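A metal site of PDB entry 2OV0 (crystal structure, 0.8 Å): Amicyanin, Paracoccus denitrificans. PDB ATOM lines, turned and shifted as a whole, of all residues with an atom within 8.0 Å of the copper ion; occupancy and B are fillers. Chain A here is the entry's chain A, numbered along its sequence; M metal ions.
Residues that only touch the copper ion: Pro 52 and Met 98.
A ring nitrogen (ND1) of His 53 lies close to the side-chain sulfur (SD) of Met 98, at 3.4 Å.
A ring nitrogen (NE2) of His 53 lies close to the backbone carbonyl oxygen (O) of Met 51 (3.4 Å).
OE2 of Glu 49 sits at hydrogen-bond distance from NE2 of His 53 (2.8 Å).
The backbone carbonyl oxygen of His 53 lies within hydrogen-bond range of the backbone NH of Met 72 (2.8 Å).
NE2 of His 95 lies close to SD of Met 51 (3.6 Å).
N of Cys 92 is in hydrogen-bond range of O of Met 98 (3.2 Å).
The backbone NH of Asn 54 lies close to the side-chain sulfur of Cys 92 (3.6 Å).
The side-chain hydroxyl of Tyr 30 lies within hydrogen-bond range of the backbone NH of Cys 92.
A ring nitrogen (ND1) of His 53 is bound to the copper ion (2.0 Å).
The copper ion is bound by ND1 of His 95 (2.0 Å).
SG of Cys 92 binds the copper ion (2.2 Å).
The copper ion has three donor atoms within binding distance.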
ATOM      1  N   ILE A  25     -30.463   3.807   3.474  1.00  0.00           N
ATOM      2  CA  ILE A  25     -29.215   3.643   4.215  1.00  0.00           C
ATOM      3  C   ILE A  25     -29.544   4.091   5.664  1.00  0.00           C
ATOM      4  O   ILE A  25     -29.985   5.216   5.893  1.00  0.00           O
ATOM      5  CB  ILE A  25     -28.068   4.457   3.666  1.00  0.00           C
ATOM      6  CG1 ILE A  25     -27.966   4.350   2.136  1.00  0.00           C
ATOM      7  CG2 ILE A  25     -26.747   3.977   4.306  1.00  0.00           C
ATOM      8  CD1 ILE A  25     -26.911   5.216   1.521  1.00  0.00           C
ATOM      9  N   MET A  28     -25.792   2.420   9.651  1.00  0.00           N
ATOM     10  CA  MET A  28     -24.499   2.103   9.084  1.00  0.00           C
ATOM     11  C   MET A  28     -24.533   0.881   8.155  1.00  0.00           C
ATOM     12  O   MET A  28     -23.536   0.198   8.022  1.00  0.00           O
ATOM     13  CB  MET A  28     -23.408   1.940  10.167  1.00  0.00           C
ATOM     14  CG  MET A  28     -23.317   3.153  11.086  1.00  0.00           C
ATOM     15  SD  MET A  28     -22.805   4.677  10.284  1.00  0.00           S
ATOM     16  CE  MET A  28     -21.170   4.232   9.699  1.00  0.00           C
ATOM     17  N   LYS A  29     -25.648   0.708   7.452  1.00  0.00           N
ATOM     18  CA  LYS A  29     -25.809  -0.373   6.525  1.00  0.00           C
ATOM     19  C   LYS A  29     -26.647   0.088   5.330  1.00  0.00           C
ATOM     20  O   LYS A  29     -27.571   0.859   5.464  1.00  0.00           O
ATOM     21  CB  LYS A  29     -26.562  -1.573   7.208  1.00  0.00           C
ATOM     22  CG  LYS A  29     -25.797  -2.167   8.393  1.00  0.00           C
ATOM     23  CD  LYS A  29     -26.528  -3.286   9.133  1.00  0.00           C
ATOM     24  CE  LYS A  29     -27.291  -2.802  10.333  1.00  0.00           C
ATOM     25  NZ  LYS A  29     -27.533  -3.979  11.253  1.00  0.00           N
ATOM     26  N   TYR A  30     -26.337  -0.486   4.159  1.00  0.00           N
ATOM     27  CA  TYR A  30     -27.288  -0.412   3.045  1.00  0.00           C
ATOM     28  C   TYR A  30     -28.409  -1.404   3.370  1.00  0.00           C
ATOM     29  O   TYR A  30     -28.156  -2.589   3.584  1.00  0.00           O
ATOM     30  CB  TYR A  30     -26.588  -0.786   1.742  1.00  0.00           C
ATOM     31  CG  TYR A  30     -25.411   0.092   1.391  1.00  0.00           C
ATOM     32  CD1 TYR A  30     -25.602   1.433   1.071  1.00  0.00           C
ATOM     33  CD2 TYR A  30     -24.124  -0.402   1.339  1.00  0.00           C
ATOM     34  CE1 TYR A  30     -24.529   2.263   0.736  1.00  0.00           C
ATOM     35  CE2 TYR A  30     -23.047   0.393   0.984  1.00  0.00           C
ATOM     36  CZ  TYR A  30     -23.255   1.735   0.680  1.00  0.00           C
ATOM     37  OH  TYR A  30     -22.150   2.445   0.267  1.00  0.00           O
ATOM     38  N   ASN A  47     -30.126   8.377   2.089  1.00  0.00           N
ATOM     39  CA  ASN A  47     -29.547   8.312   3.415  1.00  0.00           C
ATOM     40  C   ASN A  47     -30.581   8.731   4.437  1.00  0.00           C
ATOM     41  O   ASN A  47     -31.099   9.846   4.396  1.00  0.00           O
ATOM     42  CB  ASN A  47     -28.321   9.214   3.471  1.00  0.00           C
ATOM     43  CG  ASN A  47     -27.591   9.017   4.800  1.00  0.00           C
ATOM     44  OD1 ASN A  47     -27.938   8.095   5.577  1.00  0.00           O
ATOM     45  ND2 ASN A  47     -26.584   9.782   5.041  1.00  0.00           N
ATOM     46  N   GLU A  49     -29.934   8.468   7.791  1.00  0.00           N
ATOM     47  CA  GLU A  49     -29.315   8.731   9.078  1.00  0.00           C
ATOM     48  C   GLU A  49     -28.371   9.886   9.020  1.00  0.00           C
ATOM     49  O   GLU A  49     -27.992  10.393   7.985  1.00  0.00           O
ATOM     50  CB  GLU A  49     -28.768   7.502   9.727  1.00  0.00           C
ATOM     51  CG  GLU A  49     -27.610   7.106   8.912  1.00  0.00           C
ATOM     52  CD  GLU A  49     -26.925   5.887   9.510  1.00  0.00           C
ATOM     53  OE1 GLU A  49     -26.923   5.656  10.659  1.00  0.00           O
ATOM     54  OE2 GLU A  49     -26.235   5.096   9.008  1.00  0.00           O
ATOM     55  N   MET A  51     -25.242  10.246   9.953  1.00  0.00           N
ATOM     56  CA  MET A  51     -23.933   9.987   9.394  1.00  0.00           C
ATOM     57  C   MET A  51     -23.967  10.086   7.854  1.00  0.00           C
ATOM     58  O   MET A  51     -24.732   9.351   7.274  1.00  0.00           O
ATOM     59  CB  MET A  51     -23.553   8.553   9.819  1.00  0.00           C
ATOM     60  CG  MET A  51     -22.246   8.122   9.214  1.00  0.00           C
ATOM     61  SD  MET A  51     -20.903   9.103   9.850  1.00  0.00           S
ATOM     62  CE  MET A  51     -20.908   8.461  11.538  1.00  0.00           C
ATOM     63  N   PRO A  52     -23.129  10.893   7.215  1.00  0.00           N
ATOM     64  CA  PRO A  52     -23.078  10.915   5.755  1.00  0.00           C
ATOM     65  C   PRO A  52     -22.534   9.603   5.172  1.00  0.00           C
ATOM     66  O   PRO A  52     -21.604   9.023   5.742  1.00  0.00           O
ATOM     67  CB  PRO A  52     -22.200  12.104   5.392  1.00  0.00           C
ATOM     68  CG  PRO A  52     -22.319  12.983   6.613  1.00  0.00           C
ATOM     69  CD  PRO A  52     -22.351  12.027   7.781  1.00  0.00           C
ATOM     70  N   HIS A  53     -23.104   9.217   4.020  1.00  0.00           N
ATOM     71  CA  HIS A  53     -22.710   8.034   3.317  1.00  0.00           C
ATOM     72  C   HIS A  53     -22.671   8.296   1.814  1.00  0.00           C
ATOM     73  O   HIS A  53     -23.362   9.189   1.342  1.00  0.00           O
ATOM     74  CB  HIS A  53     -23.737   6.893   3.547  1.00  0.00           C
ATOM     75  CG  HIS A  53     -23.883   6.458   4.966  1.00  0.00           C
ATOM     76  ND1 HIS A  53     -22.840   5.811   5.634  1.00  0.00           N
ATOM     77  CD2 HIS A  53     -24.934   6.554   5.779  1.00  0.00           C
ATOM     78  CE1 HIS A  53     -23.307   5.551   6.850  1.00  0.00           C
ATOM     79  NE2 HIS A  53     -24.537   5.957   6.965  1.00  0.00           N
ATOM     80  N   ASN A  54     -21.945   7.461   1.073  1.00  0.00           N
ATOM     81  CA  ASN A  54     -22.029   7.499  -0.381  1.00  0.00           C
ATOM     82  C   ASN A  54     -22.124   6.055  -0.889  1.00  0.00           C
ATOM     83  O   ASN A  54     -22.259   5.100  -0.121  1.00  0.00           O
ATOM     84  CB  ASN A  54     -20.904   8.273  -1.048  1.00  0.00           C
ATOM     85  CG  ASN A  54     -19.583   7.531  -1.019  1.00  0.00           C
ATOM     86  OD1 ASN A  54     -19.400   6.605  -0.215  1.00  0.00           O
ATOM     87  ND2 ASN A  54     -18.672   7.916  -1.910  1.00  0.00           N
ATOM     88  N   VAL A  55     -22.055   5.934  -2.220  1.00  0.00           N
ATOM     89  CA  VAL A  55     -21.823   4.667  -2.906  1.00  0.00           C
ATOM     90  C   VAL A  55     -20.592   4.847  -3.802  1.00  0.00           C
ATOM     91  O   VAL A  55     -20.455   5.888  -4.457  1.00  0.00           O
ATOM     92  CB  VAL A  55     -23.051   4.166  -3.685  1.00  0.00           C
ATOM     93  CG1 VAL A  55     -24.187   3.867  -2.722  1.00  0.00           C
ATOM     94  CG2 VAL A  55     -23.513   5.128  -4.763  1.00  0.00           C
ATOM     95  N   MET A  71     -21.148  12.429  -1.276  1.00  0.00           N
ATOM     96  CA  MET A  71     -21.636  12.178   0.068  1.00  0.00           C
ATOM     97  C   MET A  71     -23.057  12.714   0.216  1.00  0.00           C
ATOM     98  O   MET A  71     -23.358  13.836  -0.181  1.00  0.00           O
ATOM     99  CB  MET A  71     -20.713  12.854   1.108  1.00  0.00           C
ATOM    100  CG  MET A  71     -19.296  12.324   1.118  1.00  0.00           C
ATOM    101  SD  MET A  71     -19.115  10.539   1.259  1.00  0.00           S
ATOM    102  CE  MET A  71     -20.004  10.272   2.786  1.00  0.00           C
ATOM    103  N   MET A  72     -23.930  11.883   0.748  1.00  0.00           N
ATOM    104  CA  MET A  72     -25.303  12.220   1.042  1.00  0.00           C
ATOM    105  C   MET A  72     -25.435  12.568   2.515  1.00  0.00           C
ATOM    106  O   MET A  72     -25.145  11.710   3.368  1.00  0.00           O
ATOM    107  CB  MET A  72     -26.244  11.036   0.741  1.00  0.00           C
ATOM    108  CG  MET A  72     -26.413  10.710  -0.719  1.00  0.00           C
ATOM    109  SD  MET A  72     -27.267   9.150  -1.026  1.00  0.00           S
ATOM    110  CE  MET A  72     -25.873   7.985  -0.887  1.00  0.00           C
ATOM    111  N   HIS A  91     -19.238   0.084  -2.203  1.00  0.00           N
ATOM    112  CA  HIS A  91     -19.006   0.292  -0.782  1.00  0.00           C
ATOM    113  C   HIS A  91     -19.164   1.763  -0.481  1.00  0.00           C
ATOM    114  O   HIS A  91     -19.248   2.603  -1.390  1.00  0.00           O
ATOM    115  CB  HIS A  91     -17.618  -0.237  -0.348  1.00  0.00           C
ATOM    116  CG  HIS A  91     -16.492   0.563  -0.925  1.00  0.00           C
ATOM    117  ND1 HIS A  91     -15.998   0.411  -2.177  1.00  0.00           N
ATOM    118  CD2 HIS A  91     -15.774   1.591  -0.371  1.00  0.00           C
ATOM    119  CE1 HIS A  91     -15.010   1.257  -2.387  1.00  0.00           C
ATOM    120  NE2 HIS A  91     -14.861   1.994  -1.313  1.00  0.00           N
ATOM    121  N   CYS A  92     -19.111   2.098   0.811  1.00  0.00           N
ATOM    122  CA  CYS A  92     -19.154   3.486   1.242  1.00  0.00           C
ATOM    123  C   CYS A  92     -17.697   3.954   1.452  1.00  0.00           C
ATOM    124  O   CYS A  92     -16.930   3.314   2.146  1.00  0.00           O
ATOM    125  CB  CYS A  92     -19.957   3.595   2.535  1.00  0.00           C
ATOM    126  SG  CYS A  92     -19.922   5.300   3.130  1.00  0.00           S
ATOM    127  N   THR A  93     -17.332   5.067   0.806  1.00  0.00           N
ATOM    128  CA  THR A  93     -15.960   5.531   0.876  1.00  0.00           C
ATOM    129  C   THR A  93     -15.449   5.731   2.317  1.00  0.00           C
ATOM    130  O   THR A  93     -14.416   5.146   2.673  1.00  0.00           O
ATOM    131  CB  THR A  93     -15.779   6.796  -0.003  1.00  0.00           C
ATOM    132  OG1 THR A  93     -16.175   6.513  -1.314  1.00  0.00           O
ATOM    133  CG2 THR A  93     -14.313   7.252   0.055  1.00  0.00           C
ATOM    134  N   PRO A  94     -16.105   6.505   3.167  1.00  0.00           N
ATOM    135  CA  PRO A  94     -15.597   6.646   4.539  1.00  0.00           C
ATOM    136  C   PRO A  94     -15.772   5.392   5.390  1.00  0.00           C
ATOM    137  O   PRO A  94     -15.080   5.248   6.391  1.00  0.00           O
ATOM    138  CB  PRO A  94     -16.386   7.812   5.139  1.00  0.00           C
ATOM    139  CG  PRO A  94     -17.633   7.853   4.280  1.00  0.00           C
ATOM    140  CD  PRO A  94     -17.186   7.462   2.893  1.00  0.00           C
ATOM    141  N   HIS A  95     -16.731   4.567   5.033  1.00  0.00           N
ATOM    142  CA  HIS A  95     -17.139   3.387   5.818  1.00  0.00           C
ATOM    143  C   HIS A  95     -17.041   2.129   4.950  1.00  0.00           C
ATOM    144  O   HIS A  95     -18.065   1.542   4.630  1.00  0.00           O
ATOM    145  CB  HIS A  95     -18.539   3.528   6.365  1.00  0.00           C
ATOM    146  CG  HIS A  95     -18.779   4.814   7.075  1.00  0.00           C
ATOM    147  ND1 HIS A  95     -19.827   5.646   6.653  1.00  0.00           N
ATOM    148  CD2 HIS A  95     -18.157   5.383   8.122  1.00  0.00           C
ATOM    149  CE1 HIS A  95     -19.777   6.674   7.467  1.00  0.00           C
ATOM    150  NE2 HIS A  95     -18.768   6.582   8.311  1.00  0.00           N
ATOM    151  N   PRO A  96     -15.839   1.685   4.593  1.00  0.00           N
ATOM    152  CA  PRO A  96     -15.725   0.606   3.599  1.00  0.00           C
ATOM    153  C   PRO A  96     -16.170  -0.767   4.121  1.00  0.00           C
ATOM    154  O   PRO A  96     -16.251  -1.702   3.341  1.00  0.00           O
ATOM    155  CB  PRO A  96     -14.265   0.650   3.125  1.00  0.00           C
ATOM    156  CG  PRO A  96     -13.548   1.280   4.308  1.00  0.00           C
ATOM    157  CD  PRO A  96     -14.536   2.321   4.822  1.00  0.00           C
ATOM    158  N   PHE A  97     -16.439  -0.872   5.420  1.00  0.00           N
ATOM    159  CA  PHE A  97     -17.125  -2.070   5.914  1.00  0.00           C
ATOM    160  C   PHE A  97     -18.573  -2.143   5.409  1.00  0.00           C
ATOM    161  O   PHE A  97     -19.164  -3.220   5.535  1.00  0.00           O
ATOM    162  CB  PHE A  97     -17.070  -2.086   7.465  1.00  0.00           C
ATOM    163  CG  PHE A  97     -17.568  -0.827   8.120  1.00  0.00           C
ATOM    164  CD1 PHE A  97     -18.900  -0.591   8.298  1.00  0.00           C
ATOM    165  CD2 PHE A  97     -16.642   0.149   8.551  1.00  0.00           C
ATOM    166  CE1 PHE A  97     -19.332   0.620   8.881  1.00  0.00           C
ATOM    167  CE2 PHE A  97     -17.087   1.325   9.129  1.00  0.00           C
ATOM    168  CZ  PHE A  97     -18.428   1.551   9.305  1.00  0.00           C
ATOM    169  N   MET A  98     -19.136  -1.071   4.907  1.00  0.00           N
ATOM    170  CA  MET A  98     -20.477  -1.062   4.301  1.00  0.00           C
ATOM    171  C   MET A  98     -20.331  -1.488   2.841  1.00  0.00           C
ATOM    172  O   MET A  98     -19.692  -0.772   2.049  1.00  0.00           O
ATOM    173  CB  MET A  98     -21.096   0.338   4.309  1.00  0.00           C
ATOM    174  CG  MET A  98     -21.335   0.860   5.713  1.00  0.00           C
ATOM    175  SD  MET A  98     -21.958   2.560   5.761  1.00  0.00           S
ATOM    176  CE  MET A  98     -23.504   2.407   4.825  1.00  0.00           C
HETATM  177 CU    CU M   1     -21.009   5.382   5.002  1.00  0.00          CU
